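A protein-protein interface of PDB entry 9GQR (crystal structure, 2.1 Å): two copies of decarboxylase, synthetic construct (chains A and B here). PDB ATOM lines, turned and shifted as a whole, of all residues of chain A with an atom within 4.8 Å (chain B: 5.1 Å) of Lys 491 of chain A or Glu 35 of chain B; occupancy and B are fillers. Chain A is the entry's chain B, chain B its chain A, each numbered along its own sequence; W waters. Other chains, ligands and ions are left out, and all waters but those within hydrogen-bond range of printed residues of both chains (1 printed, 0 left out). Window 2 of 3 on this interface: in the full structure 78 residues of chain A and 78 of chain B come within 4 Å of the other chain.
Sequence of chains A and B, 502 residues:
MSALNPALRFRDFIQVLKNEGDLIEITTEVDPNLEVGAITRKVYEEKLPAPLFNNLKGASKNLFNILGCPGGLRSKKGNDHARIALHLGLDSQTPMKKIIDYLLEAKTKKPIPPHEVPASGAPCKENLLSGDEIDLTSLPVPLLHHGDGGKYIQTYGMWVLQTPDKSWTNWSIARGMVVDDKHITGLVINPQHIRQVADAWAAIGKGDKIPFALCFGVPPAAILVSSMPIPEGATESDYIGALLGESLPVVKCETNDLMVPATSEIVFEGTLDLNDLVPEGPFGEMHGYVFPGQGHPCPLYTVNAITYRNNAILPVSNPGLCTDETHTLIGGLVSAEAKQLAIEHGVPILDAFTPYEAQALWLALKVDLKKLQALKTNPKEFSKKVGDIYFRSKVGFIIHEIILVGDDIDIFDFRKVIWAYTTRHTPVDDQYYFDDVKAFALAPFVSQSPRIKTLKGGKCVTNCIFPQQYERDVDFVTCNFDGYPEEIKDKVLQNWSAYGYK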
ATOM      1  N   GLU A 487     -12.611  20.424   8.775  1.00  0.00           N
ATOM      2  CA  GLU A 487     -13.598  21.442   8.434  1.00  0.00           C
ATOM      3  C   GLU A 487     -14.344  21.940   9.664  1.00  0.00           C
ATOM      4  O   GLU A 487     -14.737  23.111   9.718  1.00  0.00           O
ATOM      5  CB  GLU A 487     -14.582  20.907   7.396  1.00  0.00           C
ATOM      6  CG  GLU A 487     -14.215  21.314   5.990  1.00  0.00           C
ATOM      7  CD  GLU A 487     -13.884  22.792   5.899  1.00  0.00           C
ATOM      8  OE1 GLU A 487     -14.818  23.618   5.955  1.00  0.00           O
ATOM      9  OE2 GLU A 487     -12.685  23.128   5.786  1.00  0.00           O
ATOM     10  N   ILE A 488     -14.541  21.078  10.660  1.00  0.00           N
ATOM     11  CA  ILE A 488     -15.181  21.521  11.891  1.00  0.00           C
ATOM     12  C   ILE A 488     -14.228  22.393  12.698  1.00  0.00           C
ATOM     13  O   ILE A 488     -14.621  23.441  13.225  1.00  0.00           O
ATOM     14  CB  ILE A 488     -15.670  20.311  12.706  1.00  0.00           C
ATOM     15  CG1 ILE A 488     -16.638  19.465  11.879  1.00  0.00           C
ATOM     16  CG2 ILE A 488     -16.322  20.770  14.000  1.00  0.00           C
ATOM     17  CD1 ILE A 488     -17.901  20.198  11.476  1.00  0.00           C
ATOM     18  N   LYS A 489     -12.960  21.981  12.801  1.00  0.00           N
ATOM     19  CA  LYS A 489     -11.987  22.758  13.561  1.00  0.00           C
ATOM     20  C   LYS A 489     -11.786  24.143  12.959  1.00  0.00           C
ATOM     21  O   LYS A 489     -11.712  25.135  13.693  1.00  0.00           O
ATOM     22  CB  LYS A 489     -10.654  22.012  13.636  1.00  0.00           C
ATOM     23  CG  LYS A 489     -10.704  20.726  14.443  1.00  0.00           C
ATOM     24  CD  LYS A 489      -9.322  20.108  14.578  1.00  0.00           C
ATOM     25  CE  LYS A 489      -8.754  19.710  13.227  1.00  0.00           C
ATOM     26  NZ  LYS A 489      -7.447  19.007  13.370  1.00  0.00           N
ATOM     27  N   ASP A 490     -11.685  24.234  11.630  1.00  0.00           N
ATOM     28  CA  ASP A 490     -11.546  25.543  10.996  1.00  0.00           C
ATOM     29  C   ASP A 490     -12.763  26.413  11.285  1.00  0.00           C
ATOM     30  O   ASP A 490     -12.630  27.589  11.640  1.00  0.00           O
ATOM     31  CB  ASP A 490     -11.340  25.396   9.484  1.00  0.00           C
ATOM     32  CG  ASP A 490     -10.027  24.727   9.137  1.00  0.00           C
ATOM     33  OD1 ASP A 490      -9.849  24.336   7.965  1.00  0.00           O
ATOM     34  OD2 ASP A 490      -9.179  24.579  10.040  1.00  0.00           O
ATOM     35  N   LYS A 491     -13.960  25.833  11.164  1.00  0.00           N
ATOM     36  CA  LYS A 491     -15.191  26.585  11.387  1.00  0.00           C
ATOM     37  C   LYS A 491     -15.208  27.221  12.772  1.00  0.00           C
ATOM     38  O   LYS A 491     -15.547  28.400  12.924  1.00  0.00           O
ATOM     39  CB  LYS A 491     -16.397  25.663  11.202  1.00  0.00           C
ATOM     40  CG  LYS A 491     -17.737  26.363  11.292  1.00  0.00           C
ATOM     41  CD  LYS A 491     -17.817  27.495  10.286  1.00  0.00           C
ATOM     42  CE  LYS A 491     -19.237  27.687   9.785  1.00  0.00           C
ATOM     43  NZ  LYS A 491     -19.337  28.863   8.881  1.00  0.00           N
ATOM     44  N   VAL A 492     -14.822  26.457  13.795  1.00  0.00           N
ATOM     45  CA  VAL A 492     -14.888  26.956  15.163  1.00  0.00           C
ATOM     46  C   VAL A 492     -13.817  28.013  15.407  1.00  0.00           C
ATOM     47  O   VAL A 492     -14.047  28.995  16.123  1.00  0.00           O
ATOM     48  CB  VAL A 492     -14.774  25.781  16.153  1.00  0.00           C
ATOM     49  CG1 VAL A 492     -14.663  26.286  17.581  1.00  0.00           C
ATOM     50  CG2 VAL A 492     -15.975  24.859  16.007  1.00  0.00           C
ATOM     51  N   LEU A 493     -12.635  27.838  14.810  1.00  0.00           N
ATOM     52  CA  LEU A 493     -11.566  28.813  15.003  1.00  0.00           C
ATOM     53  C   LEU A 493     -11.850  30.106  14.245  1.00  0.00           C
ATOM     54  O   LEU A 493     -11.562  31.198  14.749  1.00  0.00           O
ATOM     55  CB  LEU A 493     -10.226  28.215  14.575  1.00  0.00           C
ATOM     56  CG  LEU A 493      -9.727  27.046  15.428  1.00  0.00           C
ATOM     57  CD1 LEU A 493      -8.467  26.439  14.833  1.00  0.00           C
ATOM     58  CD2 LEU A 493      -9.483  27.492  16.861  1.00  0.00           C
ATOM     59  N   GLN A 494     -12.411  30.005  13.035  1.00  0.00           N
ATOM     60  CA  GLN A 494     -12.815  31.199  12.300  1.00  0.00           C
ATOM     61  C   GLN A 494     -13.799  32.038  13.104  1.00  0.00           C
ATOM     62  O   GLN A 494     -13.720  33.273  13.111  1.00  0.00           O
ATOM     63  CB  GLN A 494     -13.456  30.819  10.963  1.00  0.00           C
ATOM     64  CG  GLN A 494     -12.564  30.120   9.961  1.00  0.00           C
ATOM     65  CD  GLN A 494     -13.377  29.431   8.879  1.00  0.00           C
ATOM     66  OE1 GLN A 494     -14.595  29.600   8.802  1.00  0.00           O
ATOM     67  NE2 GLN A 494     -12.710  28.647   8.041  1.00  0.00           N
ATOM     68  N   ASN A 495     -14.738  31.382  13.782  1.00  0.00           N
ATOM     69  CA  ASN A 495     -15.846  32.052  14.446  1.00  0.00           C
ATOM     70  C   ASN A 495     -15.595  32.297  15.926  1.00  0.00           C
ATOM     71  O   ASN A 495     -16.522  32.699  16.637  1.00  0.00           O
ATOM     72  CB  ASN A 495     -17.130  31.238  14.277  1.00  0.00           C
ATOM     73  CG  ASN A 495     -17.515  31.045  12.826  1.00  0.00           C
ATOM     74  OD1 ASN A 495     -17.874  29.944  12.410  1.00  0.00           O
ATOM     75  ND2 ASN A 495     -17.444  32.116  12.047  1.00  0.00           N
ATOM     76  N   TYR A 499     -18.233  34.240  18.203  1.00  0.00           N
ATOM     77  CA  TYR A 499     -18.971  33.613  19.294  1.00  0.00           C
ATOM     78  C   TYR A 499     -19.040  34.521  20.513  1.00  0.00           C
ATOM     79  O   TYR A 499     -20.031  34.499  21.252  1.00  0.00           O
ATOM     80  CB  TYR A 499     -18.323  32.282  19.684  1.00  0.00           C
ATOM     81  CG  TYR A 499     -18.388  31.202  18.628  1.00  0.00           C
ATOM     82  CD1 TYR A 499     -19.446  31.137  17.725  1.00  0.00           C
ATOM     83  CD2 TYR A 499     -17.389  30.238  18.539  1.00  0.00           C
ATOM     84  CE1 TYR A 499     -19.504  30.143  16.762  1.00  0.00           C
ATOM     85  CE2 TYR A 499     -17.437  29.243  17.584  1.00  0.00           C
ATOM     86  CZ  TYR A 499     -18.496  29.199  16.698  1.00  0.00           C
ATOM     87  OH  TYR A 499     -18.541  28.209  15.743  1.00  0.00           O
ATOM     88  N   GLU B  29     -25.348  31.452  15.131  1.00  0.00           N
ATOM     89  CA  GLU B  29     -25.944  30.153  14.850  1.00  0.00           C
ATOM     90  C   GLU B  29     -24.876  29.069  14.915  1.00  0.00           C
ATOM     91  O   GLU B  29     -23.844  29.154  14.241  1.00  0.00           O
ATOM     92  CB  GLU B  29     -26.624  30.144  13.483  1.00  0.00           C
ATOM     93  CG  GLU B  29     -27.247  28.792  13.146  1.00  0.00           C
ATOM     94  CD  GLU B  29     -27.952  28.776  11.804  1.00  0.00           C
ATOM     95  OE1 GLU B  29     -28.889  29.579  11.611  1.00  0.00           O
ATOM     96  OE2 GLU B  29     -27.564  27.961  10.940  1.00  0.00           O
ATOM     97  N   VAL B  30     -25.121  28.056  15.741  1.00  0.00           N
ATOM     98  CA  VAL B  30     -24.200  26.945  15.935  1.00  0.00           C
ATOM     99  C   VAL B  30     -24.915  25.655  15.556  1.00  0.00           C
ATOM    100  O   VAL B  30     -26.086  25.458  15.898  1.00  0.00           O
ATOM    101  CB  VAL B  30     -23.681  26.887  17.388  1.00  0.00           C
ATOM    102  CG1 VAL B  30     -22.825  25.651  17.607  1.00  0.00           C
ATOM    103  CG2 VAL B  30     -22.891  28.148  17.715  1.00  0.00           C
ATOM    104  N   ASP B  31     -24.210  24.787  14.839  1.00  0.00           N
ATOM    105  CA  ASP B  31     -24.774  23.514  14.408  1.00  0.00           C
ATOM    106  C   ASP B  31     -24.682  22.493  15.537  1.00  0.00           C
ATOM    107  O   ASP B  31     -23.593  22.277  16.081  1.00  0.00           O
ATOM    108  CB  ASP B  31     -24.036  23.002  13.172  1.00  0.00           C
ATOM    109  CG  ASP B  31     -24.749  21.844  12.492  1.00  0.00           C
ATOM    110  OD1 ASP B  31     -25.444  21.062  13.172  1.00  0.00           O
ATOM    111  OD2 ASP B  31     -24.617  21.714  11.258  1.00  0.00           O
ATOM    112  N   PRO B  32     -25.790  21.856  15.922  1.00  0.00           N
ATOM    113  CA  PRO B  32     -25.694  20.757  16.896  1.00  0.00           C
ATOM    114  C   PRO B  32     -24.811  19.615  16.430  1.00  0.00           C
ATOM    115  O   PRO B  32     -24.224  18.918  17.267  1.00  0.00           O
ATOM    116  CB  PRO B  32     -27.154  20.311  17.061  1.00  0.00           C
ATOM    117  CG  PRO B  32     -27.952  21.523  16.719  1.00  0.00           C
ATOM    118  CD  PRO B  32     -27.188  22.218  15.629  1.00  0.00           C
ATOM    119  N   ASN B  33     -24.697  19.401  15.122  1.00  0.00           N
ATOM    120  CA  ASN B  33     -23.833  18.353  14.582  1.00  0.00           C
ATOM    121  C   ASN B  33     -22.384  18.824  14.654  1.00  0.00           C
ATOM    122  O   ASN B  33     -21.949  19.658  13.856  1.00  0.00           O
ATOM    123  CB  ASN B  33     -24.232  18.006  13.151  1.00  0.00           C
ATOM    124  CG  ASN B  33     -25.610  17.377  13.064  1.00  0.00           C
ATOM    125  OD1 ASN B  33     -25.800  16.218  13.431  1.00  0.00           O
ATOM    126  ND2 ASN B  33     -26.578  18.138  12.565  1.00  0.00           N
ATOM    127  N   LEU B  34     -21.654  18.308  15.648  1.00  0.00           N
ATOM    128  CA  LEU B  34     -20.201  18.419  15.777  1.00  0.00           C
ATOM    129  C   LEU B  34     -19.715  19.786  16.251  1.00  0.00           C
ATOM    130  O   LEU B  34     -18.756  19.858  17.028  1.00  0.00           O
ATOM    131  CB  LEU B  34     -19.516  18.054  14.457  1.00  0.00           C
ATOM    132  CG  LEU B  34     -19.573  16.568  14.100  1.00  0.00           C
ATOM    133  CD1 LEU B  34     -18.816  16.285  12.812  1.00  0.00           C
ATOM    134  CD2 LEU B  34     -19.025  15.732  15.247  1.00  0.00           C
ATOM    135  N   GLU B  35     -20.345  20.871  15.794  1.00  0.00           N
ATOM    136  CA  GLU B  35     -19.873  22.202  16.169  1.00  0.00           C
ATOM    137  C   GLU B  35     -19.922  22.403  17.679  1.00  0.00           C
ATOM    138  O   GLU B  35     -18.945  22.854  18.288  1.00  0.00           O
ATOM    139  CB  GLU B  35     -20.693  23.282  15.463  1.00  0.00           C
ATOM    140  CG  GLU B  35     -20.255  23.580  14.041  1.00  0.00           C
ATOM    141  CD  GLU B  35     -20.942  24.809  13.475  1.00  0.00           C
ATOM    142  OE1 GLU B  35     -21.457  25.625  14.271  1.00  0.00           O
ATOM    143  OE2 GLU B  35     -20.969  24.959  12.234  1.00  0.00           O
ATOM    144  N   VAL B  36     -21.065  22.088  18.297  1.00  0.00           N
ATOM    145  CA  VAL B  36     -21.196  22.211  19.747  1.00  0.00           C
ATOM    146  C   VAL B  36     -20.104  21.416  20.450  1.00  0.00           C
ATOM    147  O   VAL B  36     -19.501  21.881  21.426  1.00  0.00           O
ATOM    148  CB  VAL B  36     -22.599  21.761  20.198  1.00  0.00           C
ATOM    149  CG1 VAL B  36     -22.667  21.655  21.716  1.00  0.00           C
ATOM    150  CG2 VAL B  36     -23.659  22.722  19.682  1.00  0.00           C
ATOM    151  N   GLY B  37     -19.826  20.207  19.958  1.00  0.00           N
ATOM    152  CA  GLY B  37     -18.781  19.398  20.560  1.00  0.00           C
ATOM    153  C   GLY B  37     -17.404  20.018  20.417  1.00  0.00           C
ATOM    154  O   GLY B  37     -16.616  20.025  21.365  1.00  0.00           O
ATOM    155  N   ALA B  38     -17.097  20.548  19.231  1.00  0.00           N
ATOM    156  CA  ALA B  38     -15.795  21.175  19.020  1.00  0.00           C
ATOM    157  C   ALA B  38     -15.630  22.413  19.892  1.00  0.00           C
ATOM    158  O   ALA B  38     -14.544  22.662  20.430  1.00  0.00           O
ATOM    159  CB  ALA B  38     -15.620  21.531  17.543  1.00  0.00           C
ATOM    160  N   ILE B  39     -16.695  23.202  20.040  1.00  0.00           N
ATOM    161  CA  ILE B  39     -16.622  24.396  20.874  1.00  0.00           C
ATOM    162  C   ILE B  39     -16.414  24.019  22.334  1.00  0.00           C
ATOM    163  O   ILE B  39     -15.590  24.622  23.033  1.00  0.00           O
ATOM    164  CB  ILE B  39     -17.885  25.255  20.686  1.00  0.00           C
ATOM    165  CG1 ILE B  39     -17.996  25.731  19.238  1.00  0.00           C
ATOM    166  CG2 ILE B  39     -17.876  26.440  21.641  1.00  0.00           C
ATOM    167  CD1 ILE B  39     -19.282  26.478  18.938  1.00  0.00           C
ATOM    168  N   THR B  40     -17.152  23.017  22.819  1.00  0.00           N
ATOM    169  CA  THR B  40     -17.028  22.620  24.218  1.00  0.00           C
ATOM    170  C   THR B  40     -15.653  22.036  24.513  1.00  0.00           C
ATOM    171  O   THR B  40     -15.104  22.254  25.600  1.00  0.00           O
ATOM    172  CB  THR B  40     -18.126  21.620  24.586  1.00  0.00           C
ATOM    173  OG1 THR B  40     -18.196  20.592  23.591  1.00  0.00           O
ATOM    174  CG2 THR B  40     -19.472  22.321  24.690  1.00  0.00           C
HETATM  175  O   HOH W   1     -20.564  28.014  14.031  1.00  0.00           O
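Ile 488 of chain A touches Leu 34 of chain B (CG1 to CD1, 3.97 Å). CB of Ala 38 of chain B touches CG2 of Ile 488 of chain A, at 3.7 Å. Lys 491 of chain A touches Glu 35 of chain B (CG to OE2, 3.6 Å). Val 492 of chain A touches Ala 38 of chain B. Val 492 of chain A touches Ile 39 of chain B (CG1 to CG1, 3.8 Å). Ile 39 of chain B touches Tyr 499 of chain A (CD1 to CE2, 3.6 Å).
Water W1 lies within hydrogen-bond range of OE1 of Glu 35 of chain B (2.6 Å), OH of Tyr 499 of chain A (2.7 Å) and O of Glu 29 of chain B (3.5 Å).
Of the 12 printed residues of chain B, 4 touch a printed residue of chain A. Of the 10 printed residues of chain A, 4 touch a printed residue of chain B. Printed residues of chain A that touch a printed residue of chain B: Ile 488, Lys 491, Val 492 and Tyr 499. Hydrophobic or aromatic side chains of chain A that line the printed part of chain B: Ile 488, Val 492 and Tyr 499.
OD1 of Asn 495 of chain A lies close to O of Lys 491 of chain A, 2.8 Å away. The side-chain carboxylate of Glu 35 of chain B lies within hydrogen-bond range of the backbone NH of Asp 31 of chain B (2.9 Å).
Of the printed residues of chain B, Ile 488 of chain A touches Leu 34 and Ala 38. Lys 491 of chain A touches one residue of chain B. Of the printed residues of chain B, Val 492 of chain A touches Ala 38 (3.7 Å) and Ile 39 (3.8 Å). Leu 493 of chain A touches none of the printed residues of chain B. Of the printed residues of chain B, Tyr 499 of chain A touches Ile 39. Printed residues of chain A within 4 Å of Leu 34 of chain B: Ile 488. Glu 35 of chain B touches one residue of chain A. The nearest printed residue of chain B that does not touch Lys 491 of chain A is Glu 29 of chain B (6.6 Å). The nearest printed residue of chain B that does not touch Ile 488 of chain A is Glu 35 of chain B (4.4 Å).
No position is printed for both chains. Of the 6 pairs that touch across the chains among the printed residues, none has its exchanged pair printed and touching as well.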
